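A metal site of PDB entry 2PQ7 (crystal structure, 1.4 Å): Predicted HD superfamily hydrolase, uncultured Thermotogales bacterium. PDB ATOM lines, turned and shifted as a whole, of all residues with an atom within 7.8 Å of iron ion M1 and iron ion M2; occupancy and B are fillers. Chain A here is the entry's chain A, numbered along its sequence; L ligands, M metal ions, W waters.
Four residues have an atom within 4 Å of iron ion M2: His 37, His 66, Asp 67 and Asp 132. The nearest printed residue that does not touch iron ion M2 is Val 41 (4.6 Å).
Iron ion M2 is bound by water W1, OD2 of Asp 67, OD1 of Asp 132, NE2 of His 37, NE2 of His 66 and O4 of LIG L1. Iron ion M2 has six donor atoms within binding distance.
Iron ion M1 is bound by water W1 (2.0 Å), OD1 of Asp 67 (2.0 Å), O3 of LIG L1 (2.1 Å), O3 of LG2 L2 (2.1 Å), NE2 of His 112 (2.2 Å) and NE2 of His 80 (2.2 Å).
The side-chain carboxylate (OD2) of Asp 135 lies within hydrogen-bond range of a ring nitrogen (ND1) of His 37 (2.8 Å). The backbone carbonyl oxygen of Ile 109 sits at hydrogen-bond distance from a ring nitrogen (ND1) of His 112, at 2.8 Å. ND1 of His 80 lies within hydrogen-bond range of OE1 of Glu 73 (2.7 Å). ND1 of His 66 is in hydrogen-bond range of O of Ala 63, at 2.7 Å.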
ATOM      1  N   ALA A  32      -3.549  -3.944  -1.029  1.00  0.00           N
ATOM      2  CA  ALA A  32      -4.383  -3.580   0.094  1.00  0.00           C
ATOM      3  C   ALA A  32      -5.900  -3.669  -0.234  1.00  0.00           C
ATOM      4  O   ALA A  32      -6.745  -3.676   0.674  1.00  0.00           O
ATOM      5  CB  ALA A  32      -4.032  -2.152   0.521  1.00  0.00           C
ATOM      6  N   HIS A  33      -6.247  -3.742  -1.514  1.00  0.00           N
ATOM      7  CA  HIS A  33      -7.648  -3.679  -1.902  1.00  0.00           C
ATOM      8  C   HIS A  33      -8.008  -4.543  -3.085  1.00  0.00           C
ATOM      9  O   HIS A  33      -9.038  -4.297  -3.701  1.00  0.00           O
ATOM     10  CB  HIS A  33      -7.988  -2.236  -2.296  1.00  0.00           C
ATOM     11  CG  HIS A  33      -7.679  -1.236  -1.240  1.00  0.00           C
ATOM     12  ND1 HIS A  33      -8.451  -1.079  -0.114  1.00  0.00           N
ATOM     13  CD2 HIS A  33      -6.687  -0.321  -1.146  1.00  0.00           C
ATOM     14  CE1 HIS A  33      -7.949  -0.123   0.637  1.00  0.00           C
ATOM     15  NE2 HIS A  33      -6.873   0.359   0.033  1.00  0.00           N
ATOM     16  N   ASP A  34      -7.184  -5.534  -3.413  1.00  0.00           N
ATOM     17  CA  ASP A  34      -7.426  -6.330  -4.609  1.00  0.00           C
ATOM     18  C   ASP A  34      -8.562  -7.325  -4.422  1.00  0.00           C
ATOM     19  O   ASP A  34      -9.134  -7.461  -3.336  1.00  0.00           O
ATOM     20  CB  ASP A  34      -6.123  -6.997  -5.077  1.00  0.00           C
ATOM     21  CG  ASP A  34      -5.597  -8.042  -4.114  1.00  0.00           C
ATOM     22  OD1 ASP A  34      -6.343  -8.535  -3.234  1.00  0.00           O
ATOM     23  OD2 ASP A  34      -4.406  -8.353  -4.216  1.00  0.00           O
ATOM     24  N   HIS A  37      -9.054  -9.837  -1.366  1.00  0.00           N
ATOM     25  CA  HIS A  37      -9.743  -9.319  -0.182  1.00  0.00           C
ATOM     26  C   HIS A  37     -11.264  -9.645  -0.230  1.00  0.00           C
ATOM     27  O   HIS A  37     -11.853 -10.186   0.721  1.00  0.00           O
ATOM     28  CB  HIS A  37      -9.492  -7.835  -0.002  1.00  0.00           C
ATOM     29  CG  HIS A  37     -10.469  -7.172   0.903  1.00  0.00           C
ATOM     30  ND1 HIS A  37     -10.429  -7.300   2.285  1.00  0.00           N
ATOM     31  CD2 HIS A  37     -11.570  -6.427   0.630  1.00  0.00           C
ATOM     32  CE1 HIS A  37     -11.414  -6.587   2.812  1.00  0.00           C
ATOM     33  NE2 HIS A  37     -12.124  -6.048   1.823  1.00  0.00           N
ATOM     34  N   THR A  38     -11.908  -9.342  -1.353  1.00  0.00           N
ATOM     35  CA  THR A  38     -13.341  -9.618  -1.507  1.00  0.00           C
ATOM     36  C   THR A  38     -13.666 -11.084  -1.287  1.00  0.00           C
ATOM     37  O   THR A  38     -14.617 -11.450  -0.606  1.00  0.00           O
ATOM     38  CB  THR A  38     -13.835  -9.128  -2.886  1.00  0.00           C
ATOM     39  OG1 THR A  38     -13.875  -7.678  -2.836  1.00  0.00           O
ATOM     40  CG2 THR A  38     -15.170  -9.584  -3.131  1.00  0.00           C
ATOM     41  N   VAL A  41     -13.377 -11.829   2.410  1.00  0.00           N
ATOM     42  CA  VAL A  41     -14.543 -11.238   3.118  1.00  0.00           C
ATOM     43  C   VAL A  41     -15.782 -12.121   2.911  1.00  0.00           C
ATOM     44  O   VAL A  41     -16.556 -12.385   3.832  1.00  0.00           O
ATOM     45  CB  VAL A  41     -14.766  -9.776   2.717  1.00  0.00           C
ATOM     46  CG1 VAL A  41     -16.077  -9.205   3.378  1.00  0.00           C
ATOM     47  CG2 VAL A  41     -13.598  -8.943   3.171  1.00  0.00           C
ATOM     48  N   ALA A  63     -21.103  -9.174   0.639  1.00  0.00           N
ATOM     49  CA  ALA A  63     -19.658  -9.310   0.667  1.00  0.00           C
ATOM     50  C   ALA A  63     -19.029  -9.265  -0.718  1.00  0.00           C
ATOM     51  O   ALA A  63     -18.009  -8.641  -0.921  1.00  0.00           O
ATOM     52  CB  ALA A  63     -19.274 -10.593   1.354  1.00  0.00           C
ATOM     53  N   HIS A  66     -19.380  -5.605  -2.012  1.00  0.00           N
ATOM     54  CA  HIS A  66     -19.162  -4.427  -1.141  1.00  0.00           C
ATOM     55  C   HIS A  66     -18.050  -3.490  -1.604  1.00  0.00           C
ATOM     56  O   HIS A  66     -18.168  -2.309  -1.452  1.00  0.00           O
ATOM     57  CB  HIS A  66     -18.962  -4.819   0.320  1.00  0.00           C
ATOM     58  CG  HIS A  66     -17.567  -5.222   0.677  1.00  0.00           C
ATOM     59  ND1 HIS A  66     -17.000  -6.405   0.271  1.00  0.00           N
ATOM     60  CD2 HIS A  66     -16.628  -4.579   1.411  1.00  0.00           C
ATOM     61  CE1 HIS A  66     -15.756  -6.470   0.724  1.00  0.00           C
ATOM     62  NE2 HIS A  66     -15.505  -5.367   1.428  1.00  0.00           N
ATOM     63  N   ASP A  67     -16.993  -4.040  -2.192  1.00  0.00           N
ATOM     64  CA  ASP A  67     -15.893  -3.243  -2.708  1.00  0.00           C
ATOM     65  C   ASP A  67     -15.809  -3.233  -4.257  1.00  0.00           C
ATOM     66  O   ASP A  67     -14.750  -2.910  -4.797  1.00  0.00           O
ATOM     67  CB  ASP A  67     -14.599  -3.764  -2.128  1.00  0.00           C
ATOM     68  CG  ASP A  67     -14.362  -3.306  -0.685  1.00  0.00           C
ATOM     69  OD1 ASP A  67     -14.930  -2.297  -0.177  1.00  0.00           O
ATOM     70  OD2 ASP A  67     -13.516  -3.961  -0.013  1.00  0.00           O
ATOM     71  N   ILE A  68     -16.937  -3.529  -4.934  1.00  0.00           N
ATOM     72  CA  ILE A  68     -16.910  -3.626  -6.387  1.00  0.00           C
ATOM     73  C   ILE A  68     -16.593  -2.282  -7.039  1.00  0.00           C
ATOM     74  O   ILE A  68     -16.029  -2.254  -8.126  1.00  0.00           O
ATOM     75  CB  ILE A  68     -18.160  -4.280  -6.955  1.00  0.00           C
ATOM     76  CG1 ILE A  68     -17.862  -4.887  -8.356  1.00  0.00           C
ATOM     77  CG2 ILE A  68     -19.367  -3.317  -6.995  1.00  0.00           C
ATOM     78  CD1 ILE A  68     -19.029  -5.533  -9.021  1.00  0.00           C
ATOM     79  N   ARG A  70     -14.407  -0.168  -5.653  1.00  0.00           N
ATOM     80  CA  ARG A  70     -13.075   0.270  -5.184  1.00  0.00           C
ATOM     81  C   ARG A  70     -12.174   0.714  -6.338  1.00  0.00           C
ATOM     82  O   ARG A  70     -11.519   1.740  -6.254  1.00  0.00           O
ATOM     83  CB  ARG A  70     -12.361  -0.802  -4.343  1.00  0.00           C
ATOM     84  CG  ARG A  70     -12.457  -0.621  -2.891  1.00  0.00           C
ATOM     85  CD  ARG A  70     -11.529   0.461  -2.447  1.00  0.00           C
ATOM     86  NE  ARG A  70     -11.554   0.621  -1.000  1.00  0.00           N
ATOM     87  CZ  ARG A  70     -10.919   1.580  -0.352  1.00  0.00           C
ATOM     88  NH1 ARG A  70     -10.211   2.485  -1.013  1.00  0.00           N
ATOM     89  NH2 ARG A  70     -11.004   1.654   0.978  1.00  0.00           N
ATOM     90  N   GLU A  73     -13.254   4.039  -7.358  1.00  0.00           N
ATOM     91  CA  GLU A  73     -12.839   5.104  -6.403  1.00  0.00           C
ATOM     92  C   GLU A  73     -11.370   5.480  -6.649  1.00  0.00           C
ATOM     93  O   GLU A  73     -11.028   6.651  -6.579  1.00  0.00           O
ATOM     94  CB  GLU A  73     -13.012   4.637  -4.956  1.00  0.00           C
ATOM     95  CG  GLU A  73     -12.593   5.709  -3.967  1.00  0.00           C
ATOM     96  CD  GLU A  73     -12.851   5.379  -2.518  1.00  0.00           C
ATOM     97  OE1 GLU A  73     -13.806   4.677  -2.220  1.00  0.00           O
ATOM     98  OE2 GLU A  73     -12.103   5.873  -1.667  1.00  0.00           O
ATOM     99  N   ASP A  79     -16.748   7.940  -3.536  1.00  0.00           N
ATOM    100  CA  ASP A  79     -16.801   6.982  -2.442  1.00  0.00           C
ATOM    101  C   ASP A  79     -17.371   5.598  -2.882  1.00  0.00           C
ATOM    102  O   ASP A  79     -18.505   5.537  -3.343  1.00  0.00           O
ATOM    103  CB  ASP A  79     -17.665   7.509  -1.312  1.00  0.00           C
ATOM    104  CG  ASP A  79     -18.001   6.457  -0.252  1.00  0.00           C
ATOM    105  OD1 ASP A  79     -17.161   5.661   0.199  1.00  0.00           O
ATOM    106  OD2 ASP A  79     -19.165   6.428   0.165  1.00  0.00           O
ATOM    107  N   HIS A  80     -16.589   4.561  -2.694  1.00  0.00           N
ATOM    108  CA  HIS A  80     -16.958   3.229  -3.156  1.00  0.00           C
ATOM    109  C   HIS A  80     -18.180   2.627  -2.418  1.00  0.00           C
ATOM    110  O   HIS A  80     -18.919   1.788  -2.980  1.00  0.00           O
ATOM    111  CB  HIS A  80     -15.791   2.259  -3.127  1.00  0.00           C
ATOM    112  CG  HIS A  80     -15.393   1.755  -1.779  1.00  0.00           C
ATOM    113  ND1 HIS A  80     -14.634   2.498  -0.879  1.00  0.00           N
ATOM    114  CD2 HIS A  80     -15.624   0.569  -1.171  1.00  0.00           C
ATOM    115  CE1 HIS A  80     -14.434   1.788   0.212  1.00  0.00           C
ATOM    116  NE2 HIS A  80     -15.003   0.603   0.059  1.00  0.00           N
ATOM    117  N   ALA A  81     -18.390   3.027  -1.171  1.00  0.00           N
ATOM    118  CA  ALA A  81     -19.548   2.515  -0.431  1.00  0.00           C
ATOM    119  C   ALA A  81     -20.851   3.048  -1.060  1.00  0.00           C
ATOM    120  O   ALA A  81     -21.838   2.313  -1.262  1.00  0.00           O
ATOM    121  CB  ALA A  81     -19.420   2.903   1.055  1.00  0.00           C
ATOM    122  N   ILE A 109     -24.000  -2.307   2.041  1.00  0.00           N
ATOM    123  CA  ILE A 109     -22.813  -1.851   1.354  1.00  0.00           C
ATOM    124  C   ILE A 109     -22.588  -0.381   1.630  1.00  0.00           C
ATOM    125  O   ILE A 109     -21.486   0.101   1.844  1.00  0.00           O
ATOM    126  CB  ILE A 109     -22.951  -2.108  -0.162  1.00  0.00           C
ATOM    127  CG1 ILE A 109     -22.999  -3.633  -0.428  1.00  0.00           C
ATOM    128  CG2 ILE A 109     -21.819  -1.399  -0.975  1.00  0.00           C
ATOM    129  CD1 ILE A 109     -23.382  -4.004  -1.857  1.00  0.00           C
ATOM    130  N   HIS A 112     -20.874   0.132   5.087  1.00  0.00           N
ATOM    131  CA  HIS A 112     -19.736  -0.672   5.509  1.00  0.00           C
ATOM    132  C   HIS A 112     -18.436  -0.034   5.984  1.00  0.00           C
ATOM    133  O   HIS A 112     -17.702  -0.686   6.695  1.00  0.00           O
ATOM    134  CB  HIS A 112     -19.437  -1.792   4.486  1.00  0.00           C
ATOM    135  CG  HIS A 112     -18.499  -1.408   3.374  1.00  0.00           C
ATOM    136  ND1 HIS A 112     -18.926  -0.908   2.168  1.00  0.00           N
ATOM    137  CD2 HIS A 112     -17.152  -1.511   3.285  1.00  0.00           C
ATOM    138  CE1 HIS A 112     -17.874  -0.693   1.390  1.00  0.00           C
ATOM    139  NE2 HIS A 112     -16.781  -1.059   2.045  1.00  0.00           N
ATOM    140  N   ARG A 113     -18.191   1.208   5.607  1.00  0.00           N
ATOM    141  CA  ARG A 113     -16.955   1.868   6.092  1.00  0.00           C
ATOM    142  C   ARG A 113     -17.062   2.341   7.547  1.00  0.00           C
ATOM    143  O   ARG A 113     -18.172   2.668   7.991  1.00  0.00           O
ATOM    144  CB  ARG A 113     -16.577   3.065   5.247  1.00  0.00           C
ATOM    145  CG  ARG A 113     -16.357   2.838   3.798  1.00  0.00           C
ATOM    146  CD  ARG A 113     -15.035   3.546   3.422  1.00  0.00           C
ATOM    147  NE  ARG A 113     -15.147   4.479   2.321  1.00  0.00           N
ATOM    148  CZ  ARG A 113     -14.107   4.947   1.636  1.00  0.00           C
ATOM    149  NH1 ARG A 113     -12.861   4.553   1.911  1.00  0.00           N
ATOM    150  NH2 ARG A 113     -14.320   5.810   0.646  1.00  0.00           N
ATOM    151  N   LEU A 128     -21.535  -7.902   7.392  1.00  0.00           N
ATOM    152  CA  LEU A 128     -20.623  -7.444   6.346  1.00  0.00           C
ATOM    153  C   LEU A 128     -19.465  -6.700   6.957  1.00  0.00           C
ATOM    154  O   LEU A 128     -18.314  -6.946   6.603  1.00  0.00           O
ATOM    155  CB  LEU A 128     -21.332  -6.547   5.332  1.00  0.00           C
ATOM    156  CG  LEU A 128     -20.414  -5.922   4.287  1.00  0.00           C
ATOM    157  CD1 LEU A 128     -19.656  -6.992   3.462  1.00  0.00           C
ATOM    158  CD2 LEU A 128     -21.191  -5.011   3.381  1.00  0.00           C
ATOM    159  N   ALA A 131     -17.165  -9.095   8.737  1.00  0.00           N
ATOM    160  CA  ALA A 131     -16.457  -9.906   7.752  1.00  0.00           C
ATOM    161  C   ALA A 131     -15.306  -9.133   7.073  1.00  0.00           C
ATOM    162  O   ALA A 131     -14.211  -9.679   6.823  1.00  0.00           O
ATOM    163  CB  ALA A 131     -17.442 -10.393   6.708  1.00  0.00           C
ATOM    164  N   ASP A 132     -15.570  -7.865   6.805  1.00  0.00           N
ATOM    165  CA  ASP A 132     -14.602  -6.960   6.167  1.00  0.00           C
ATOM    166  C   ASP A 132     -13.463  -6.709   7.148  1.00  0.00           C
ATOM    167  O   ASP A 132     -12.279  -6.895   6.813  1.00  0.00           O
ATOM    168  CB  ASP A 132     -15.308  -5.667   5.815  1.00  0.00           C
ATOM    169  CG  ASP A 132     -14.475  -4.720   4.956  1.00  0.00           C
ATOM    170  OD1 ASP A 132     -13.796  -5.216   4.007  1.00  0.00           O
ATOM    171  OD2 ASP A 132     -14.527  -3.507   5.217  1.00  0.00           O
ATOM    172  N   ARG A 133     -13.823  -6.336   8.379  1.00  0.00           N
ATOM    173  CA  ARG A 133     -12.789  -5.951   9.336  1.00  0.00           C
ATOM    174  C   ARG A 133     -11.968  -7.119   9.806  1.00  0.00           C
ATOM    175  O   ARG A 133     -10.768  -6.951  10.111  1.00  0.00           O
ATOM    176  CB  ARG A 133     -13.373  -5.173  10.518  1.00  0.00           C
ATOM    177  CG  ARG A 133     -14.015  -3.876  10.109  1.00  0.00           C
ATOM    178  CD  ARG A 133     -14.772  -3.171  11.193  1.00  0.00           C
ATOM    179  NE  ARG A 133     -13.862  -2.827  12.283  1.00  0.00           N
ATOM    180  CZ  ARG A 133     -13.742  -3.455  13.458  1.00  0.00           C
ATOM    181  NH1 ARG A 133     -14.546  -4.458  13.831  1.00  0.00           N
ATOM    182  NH2 ARG A 133     -12.826  -3.017  14.314  1.00  0.00           N
ATOM    183  N   ASP A 135     -10.596  -9.182   8.059  1.00  0.00           N
ATOM    184  CA  ASP A 135      -9.502  -9.373   7.095  1.00  0.00           C
ATOM    185  C   ASP A 135      -8.217  -8.633   7.462  1.00  0.00           C
ATOM    186  O   ASP A 135      -7.185  -8.887   6.859  1.00  0.00           O
ATOM    187  CB  ASP A 135      -9.957  -9.012   5.671  1.00  0.00           C
ATOM    188  CG  ASP A 135      -9.048  -9.636   4.614  1.00  0.00           C
ATOM    189  OD1 ASP A 135      -8.799 -10.865   4.691  1.00  0.00           O
ATOM    190  OD2 ASP A 135      -8.632  -8.887   3.724  1.00  0.00           O
HETATM  191  P1  LIG L   1     -11.442  -1.920   1.570  1.00  0.00           P
HETATM  192  O1  LIG L   1     -10.553  -1.041   2.406  1.00  0.00           O
HETATM  193  O2  LIG L   1     -10.620  -2.349   0.343  1.00  0.00           O
HETATM  194  O3  LIG L   1     -12.626  -1.071   1.104  1.00  0.00           O
HETATM  195  O4  LIG L   1     -11.734  -3.203   2.343  1.00  0.00           O
HETATM  196  P1  LG2 L   2     -13.233   0.433   3.974  1.00  0.00           P
HETATM  197  O1  LG2 L   2     -12.146   1.398   3.491  1.00  0.00           O
HETATM  198  O2  LG2 L   2     -12.629  -0.904   4.349  1.00  0.00           O
HETATM  199  O3  LG2 L   2     -14.316   0.249   2.924  1.00  0.00           O
HETATM  200  O4  LG2 L   2     -13.849   1.057   5.203  1.00  0.00           O
HETATM  201 FE    FE M   1     -14.660  -1.120   1.419  1.00  0.00          FE
HETATM  202 FE    FE M   2     -13.561  -4.454   2.033  1.00  0.00          FE
HETATM  203  O   HOH W   1     -14.446  -2.680   2.645  1.00  0.00           O
